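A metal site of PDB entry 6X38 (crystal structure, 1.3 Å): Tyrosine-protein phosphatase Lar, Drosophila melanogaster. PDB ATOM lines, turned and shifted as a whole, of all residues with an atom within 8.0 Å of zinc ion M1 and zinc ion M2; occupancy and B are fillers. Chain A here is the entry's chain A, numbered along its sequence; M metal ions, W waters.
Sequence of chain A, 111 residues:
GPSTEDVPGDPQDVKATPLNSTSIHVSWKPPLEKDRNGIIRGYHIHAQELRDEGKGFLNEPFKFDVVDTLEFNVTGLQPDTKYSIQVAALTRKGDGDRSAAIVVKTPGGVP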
ATOM      1  N   GLY A  42      17.285   0.436  12.291  1.00  0.00           N
ATOM      2  CA  GLY A  42      18.718   0.692  12.336  1.00  0.00           C
ATOM      3  C   GLY A  42      19.049   1.947  13.091  1.00  0.00           C
ATOM      4  O   GLY A  42      18.374   2.983  12.947  1.00  0.00           O
ATOM      5  N   TYR A  43      20.145   1.902  13.854  1.00  0.00           N
ATOM      6  CA  TYR A  43      20.661   3.054  14.584  1.00  0.00           C
ATOM      7  C   TYR A  43      22.185   3.093  14.422  1.00  0.00           C
ATOM      8  O   TYR A  43      22.836   2.081  14.133  1.00  0.00           O
ATOM      9  CB  TYR A  43      20.358   2.927  16.126  1.00  0.00           C
ATOM     10  CG  TYR A  43      18.873   2.992  16.409  1.00  0.00           C
ATOM     11  CD1 TYR A  43      18.104   1.842  16.398  1.00  0.00           C
ATOM     12  CD2 TYR A  43      18.277   4.156  16.765  1.00  0.00           C
ATOM     13  CE1 TYR A  43      16.732   1.892  16.672  1.00  0.00           C
ATOM     14  CE2 TYR A  43      16.918   4.221  17.012  1.00  0.00           C
ATOM     15  CZ  TYR A  43      16.159   3.086  16.984  1.00  0.00           C
ATOM     16  OH  TYR A  43      14.793   3.196  17.294  1.00  0.00           O
ATOM     17  N   HIS A  44      22.745   4.272  14.645  1.00  0.00           N
ATOM     18  CA  HIS A  44      24.183   4.456  14.895  1.00  0.00           C
ATOM     19  C   HIS A  44      24.384   4.811  16.372  1.00  0.00           C
ATOM     20  O   HIS A  44      23.621   5.615  16.930  1.00  0.00           O
ATOM     21  CB  HIS A  44      24.801   5.588  14.100  1.00  0.00           C
ATOM     22  CG  HIS A  44      25.090   5.243  12.702  1.00  0.00           C
ATOM     23  ND1 HIS A  44      25.504   6.218  11.807  1.00  0.00           N
ATOM     24  CD2 HIS A  44      25.057   4.054  12.037  1.00  0.00           C
ATOM     25  CE1 HIS A  44      25.729   5.586  10.645  1.00  0.00           C
ATOM     26  NE2 HIS A  44      25.474   4.306  10.745  1.00  0.00           N
ATOM     27  N   ILE A  45      25.409   4.235  16.968  1.00  0.00           N
ATOM     28  CA  ILE A  45      25.990   4.771  18.211  1.00  0.00           C
ATOM     29  C   ILE A  45      27.286   5.440  17.845  1.00  0.00           C
ATOM     30  O   ILE A  45      28.161   4.827  17.227  1.00  0.00           O
ATOM     31  CB  ILE A  45      26.183   3.679  19.265  1.00  0.00           C
ATOM     32  CG1 ILE A  45      24.883   2.971  19.597  1.00  0.00           C
ATOM     33  CG2 ILE A  45      26.843   4.294  20.505  1.00  0.00           C
ATOM     34  CD1 ILE A  45      25.096   1.689  20.332  1.00  0.00           C
ATOM     35  N   HIS A  46      27.430   6.674  18.273  1.00  0.00           N
ATOM     36  CA  HIS A  46      28.628   7.463  18.032  1.00  0.00           C
ATOM     37  C   HIS A  46      29.320   7.659  19.370  1.00  0.00           C
ATOM     38  O   HIS A  46      28.680   8.117  20.318  1.00  0.00           O
ATOM     39  CB  HIS A  46      28.233   8.775  17.350  1.00  0.00           C
ATOM     40  CG  HIS A  46      27.861   8.619  15.888  1.00  0.00           C
ATOM     41  ND1 HIS A  46      28.817   8.502  14.916  1.00  0.00           N
ATOM     42  CD2 HIS A  46      26.672   8.596  15.229  1.00  0.00           C
ATOM     43  CE1 HIS A  46      28.249   8.385  13.723  1.00  0.00           C
ATOM     44  NE2 HIS A  46      26.949   8.450  13.893  1.00  0.00           N
ATOM     45  N   PHE A  62      34.463   6.717  17.246  1.00  0.00           N
ATOM     46  CA  PHE A  62      33.953   5.405  16.853  1.00  0.00           C
ATOM     47  C   PHE A  62      32.513   5.547  16.403  1.00  0.00           C
ATOM     48  O   PHE A  62      31.721   6.338  16.962  1.00  0.00           O
ATOM     49  CB  PHE A  62      33.986   4.427  18.055  1.00  0.00           C
ATOM     50  CG  PHE A  62      35.343   4.075  18.573  1.00  0.00           C
ATOM     51  CD1 PHE A  62      36.015   4.924  19.454  1.00  0.00           C
ATOM     52  CD2 PHE A  62      35.919   2.860  18.249  1.00  0.00           C
ATOM     53  CE1 PHE A  62      37.272   4.567  19.932  1.00  0.00           C
ATOM     54  CE2 PHE A  62      37.167   2.499  18.724  1.00  0.00           C
ATOM     55  CZ  PHE A  62      37.842   3.368  19.566  1.00  0.00           C
ATOM     56  N   LYS A  63      32.123   4.713  15.447  1.00  0.00           N
ATOM     57  CA  LYS A  63      30.724   4.569  15.054  1.00  0.00           C
ATOM     58  C   LYS A  63      30.397   3.104  15.038  1.00  0.00           C
ATOM     59  O   LYS A  63      31.181   2.294  14.570  1.00  0.00           O
ATOM     60  CB  LYS A  63      30.516   5.186  13.644  1.00  0.00           C
ATOM     61  CG  LYS A  63      29.067   5.099  13.136  1.00  0.00           C
ATOM     62  CD  LYS A  63      28.819   3.878  12.323  1.00  0.00           C
ATOM     63  CE  LYS A  63      29.348   4.095  10.915  1.00  0.00           C
ATOM     64  NZ  LYS A  63      29.631   2.793  10.189  1.00  0.00           N
ATOM     65  N   PHE A  64      29.227   2.766  15.524  1.00  0.00           N
ATOM     66  CA  PHE A  64      28.736   1.394  15.560  1.00  0.00           C
ATOM     67  C   PHE A  64      27.377   1.316  14.901  1.00  0.00           C
ATOM     68  O   PHE A  64      26.477   2.066  15.280  1.00  0.00           O
ATOM     69  CB  PHE A  64      28.633   0.890  17.012  1.00  0.00           C
ATOM     70  CG  PHE A  64      29.960   0.915  17.741  1.00  0.00           C
ATOM     71  CD1 PHE A  64      30.366   2.053  18.366  1.00  0.00           C
ATOM     72  CD2 PHE A  64      30.786  -0.181  17.758  1.00  0.00           C
ATOM     73  CE1 PHE A  64      31.595   2.125  19.007  1.00  0.00           C
ATOM     74  CE2 PHE A  64      32.020  -0.128  18.411  1.00  0.00           C
ATOM     75  CZ  PHE A  64      32.400   1.032  19.049  1.00  0.00           C
ATOM     76  N   ASP A  65      27.227   0.438  13.949  1.00  0.00           N
ATOM     77  CA  ASP A  65      25.935   0.152  13.360  1.00  0.00           C
ATOM     78  C   ASP A  65      25.193  -0.870  14.158  1.00  0.00           C
ATOM     79  O   ASP A  65      25.740  -1.915  14.535  1.00  0.00           O
ATOM     80  CB  ASP A  65      26.080  -0.413  11.950  1.00  0.00           C
ATOM     81  CG  ASP A  65      26.349   0.644  10.986  1.00  0.00           C
ATOM     82  OD1 ASP A  65      25.383   1.203  10.375  1.00  0.00           O
ATOM     83  OD2 ASP A  65      27.543   0.979  10.757  1.00  0.00           O
ATOM     84  N   VAL A  66      23.938  -0.599  14.457  1.00  0.00           N
ATOM     85  CA  VAL A  66      23.054  -1.480  15.233  1.00  0.00           C
ATOM     86  C   VAL A  66      21.847  -1.789  14.375  1.00  0.00           C
ATOM     87  O   VAL A  66      21.284  -0.881  13.745  1.00  0.00           O
ATOM     88  CB  VAL A  66      22.640  -0.779  16.553  1.00  0.00           C
ATOM     89  CG1 VAL A  66      21.869  -1.761  17.490  1.00  0.00           C
ATOM     90  CG2 VAL A  66      23.903  -0.255  17.273  1.00  0.00           C
ATOM     91  N   VAL A  67      21.479  -3.047  14.286  1.00  0.00           N
ATOM     92  CA  VAL A  67      20.309  -3.486  13.546  1.00  0.00           C
ATOM     93  C   VAL A  67      19.423  -4.337  14.427  1.00  0.00           C
ATOM     94  O   VAL A  67      19.904  -5.272  15.063  1.00  0.00           O
ATOM     95  CB  VAL A  67      20.706  -4.289  12.288  1.00  0.00           C
ATOM     96  CG1 VAL A  67      19.465  -4.811  11.605  1.00  0.00           C
ATOM     97  CG2 VAL A  67      21.545  -3.419  11.342  1.00  0.00           C
ATOM     98  N   GLN A  86      26.383   9.162  21.916  1.00  0.00           N
ATOM     99  CA  GLN A  86      25.141   9.616  21.313  1.00  0.00           C
ATOM    100  C   GLN A  86      24.580   8.510  20.437  1.00  0.00           C
ATOM    101  O   GLN A  86      25.339   7.755  19.819  1.00  0.00           O
ATOM    102  CB  GLN A  86      25.369  10.910  20.518  1.00  0.00           C
ATOM    103  CG  GLN A  86      25.722  12.096  21.380  1.00  0.00           C
ATOM    104  CD  GLN A  86      25.861  13.369  20.569  1.00  0.00           C
ATOM    105  OE1 GLN A  86      26.819  13.515  19.844  1.00  0.00           O
ATOM    106  NE2 GLN A  86      24.909  14.250  20.659  1.00  0.00           N
ATOM    107  N   VAL A  87      23.268   8.479  20.285  1.00  0.00           N
ATOM    108  CA  VAL A  87      22.594   7.489  19.446  1.00  0.00           C
ATOM    109  C   VAL A  87      21.738   8.268  18.442  1.00  0.00           C
ATOM    110  O   VAL A  87      21.125   9.280  18.795  1.00  0.00           O
ATOM    111  CB  VAL A  87      21.725   6.545  20.306  1.00  0.00           C
ATOM    112  CG1 VAL A  87      21.154   5.424  19.447  1.00  0.00           C
ATOM    113  CG2 VAL A  87      22.501   5.962  21.475  1.00  0.00           C
ATOM    114  N   ALA A  88      21.629   7.730  17.210  1.00  0.00           N
ATOM    115  CA  ALA A  88      20.800   8.344  16.194  1.00  0.00           C
ATOM    116  C   ALA A  88      20.083   7.261  15.410  1.00  0.00           C
ATOM    117  O   ALA A  88      20.691   6.229  15.107  1.00  0.00           O
ATOM    118  CB  ALA A  88      21.612   9.211  15.230  1.00  0.00           C
ATOM    119  N   ALA A  89      18.846   7.491  15.024  1.00  0.00           N
ATOM    120  CA  ALA A  89      18.171   6.634  14.058  1.00  0.00           C
ATOM    121  C   ALA A  89      18.692   6.883  12.659  1.00  0.00           C
ATOM    122  O   ALA A  89      19.131   7.977  12.341  1.00  0.00           O
ATOM    123  CB  ALA A  89      16.671   6.971  14.082  1.00  0.00           C
ATOM    124  N   LEU A  90      18.632   5.866  11.819  1.00  0.00           N
ATOM    125  CA  LEU A  90      19.068   5.999  10.431  1.00  0.00           C
ATOM    126  C   LEU A  90      17.924   6.355   9.527  1.00  0.00           C
ATOM    127  O   LEU A  90      16.850   5.792   9.652  1.00  0.00           O
ATOM    128  CB  LEU A  90      19.728   4.692   9.980  1.00  0.00           C
ATOM    129  CG  LEU A  90      20.973   4.345  10.810  1.00  0.00           C
ATOM    130  CD1 LEU A  90      21.598   3.013  10.400  1.00  0.00           C
ATOM    131  CD2 LEU A  90      22.010   5.436  10.759  1.00  0.00           C
ATOM    132  N   GLY A  94      20.577  10.443   6.015  1.00  0.00           N
ATOM    133  CA  GLY A  94      21.634  10.260   6.967  1.00  0.00           C
ATOM    134  C   GLY A  94      21.082  10.008   8.357  1.00  0.00           C
ATOM    135  O   GLY A  94      19.962   9.459   8.500  1.00  0.00           O
ATOM    136  N   ASP A  95      21.826  10.369   9.355  1.00  0.00           N
ATOM    137  CA  ASP A  95      21.331  10.163  10.711  1.00  0.00           C
ATOM    138  C   ASP A  95      20.206  11.145  11.008  1.00  0.00           C
ATOM    139  O   ASP A  95      20.234  12.295  10.553  1.00  0.00           O
ATOM    140  CB  ASP A  95      22.456  10.370  11.727  1.00  0.00           C
ATOM    141  CG  ASP A  95      23.533   9.294  11.651  1.00  0.00           C
ATOM    142  OD1 ASP A  95      23.650   8.535  10.659  1.00  0.00           O
ATOM    143  OD2 ASP A  95      24.399   9.293  12.527  1.00  0.00           O
ATOM    144  N   GLY A  96      19.219  10.704  11.801  1.00  0.00           N
ATOM    145  CA  GLY A  96      18.288  11.623  12.421  1.00  0.00           C
ATOM    146  C   GLY A  96      18.995  12.310  13.585  1.00  0.00           C
ATOM    147  O   GLY A  96      20.173  12.143  13.843  1.00  0.00           O
ATOM    148  N   ARG A  98      20.621  13.337  16.933  1.00  0.00           N
ATOM    149  CA  ARG A  98      21.313  12.572  17.953  1.00  0.00           C
ATOM    150  C   ARG A  98      20.729  12.823  19.332  1.00  0.00           C
ATOM    151  O   ARG A  98      20.321  13.938  19.646  1.00  0.00           O
ATOM    152  CB  ARG A  98      22.793  12.948  17.997  1.00  0.00           C
ATOM    153  CG  ARG A  98      23.556  12.601  16.748  1.00  0.00           C
ATOM    154  CD  ARG A  98      25.025  12.920  16.984  1.00  0.00           C
ATOM    155  NE  ARG A  98      25.865  12.487  15.876  1.00  0.00           N
ATOM    156  CZ  ARG A  98      27.185  12.297  15.976  1.00  0.00           C
ATOM    157  NH1 ARG A  98      27.808  12.438  17.145  1.00  0.00           N
ATOM    158  NH2 ARG A  98      27.837  11.891  14.910  1.00  0.00           N
HETATM  159 ZN    ZN M   1      25.851   8.097  12.219  1.00  0.00          ZN
HETATM  160 ZN    ZN M   2      25.696   2.882   9.347  1.00  0.00          ZN
HETATM  161  O   HOH W   1      26.817   8.808  10.570  1.00  0.00           O
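The backbone NH (N) of His 46 sits at hydrogen-bond distance from the backbone carbonyl oxygen (O) of Gln 86 (2.8 Å).
The side-chain carboxylate (OD2) of Asp 65 is in salt-bridge range of the side-chain amino group (NZ) of Lys 63, at 2.8 Å.
O of Ala 88 sits at hydrogen-bond distance from N of His 44 (2.9 Å).
Three residues have an atom within 4 Å of zinc ion M1: His 44, His 46 and Asp 95.
Two residues have an atom within 4 Å of zinc ion M2: His 44 and Asp 65.
The nearest printed residue that does not touch zinc ion M2 is Lys 63 (4.03 Å).
Zinc ion M1 is bound by the side-chain carboxylate of Asp 95, a ring nitrogen (ND1) of His 44, a ring nitrogen (NE2) of His 46 and water W1.
Zinc ion M1 has four donor atoms within binding distance.
Slightly farther from zinc ion M1 lies OD1 of Asp 95 (2.7 Å).
Zinc ion M2 is bound by OD1 of Asp 65 (2.0 Å) and NE2 of His 44 (2.0 Å).
Zinc ion M2 has two donor atoms within binding distance.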
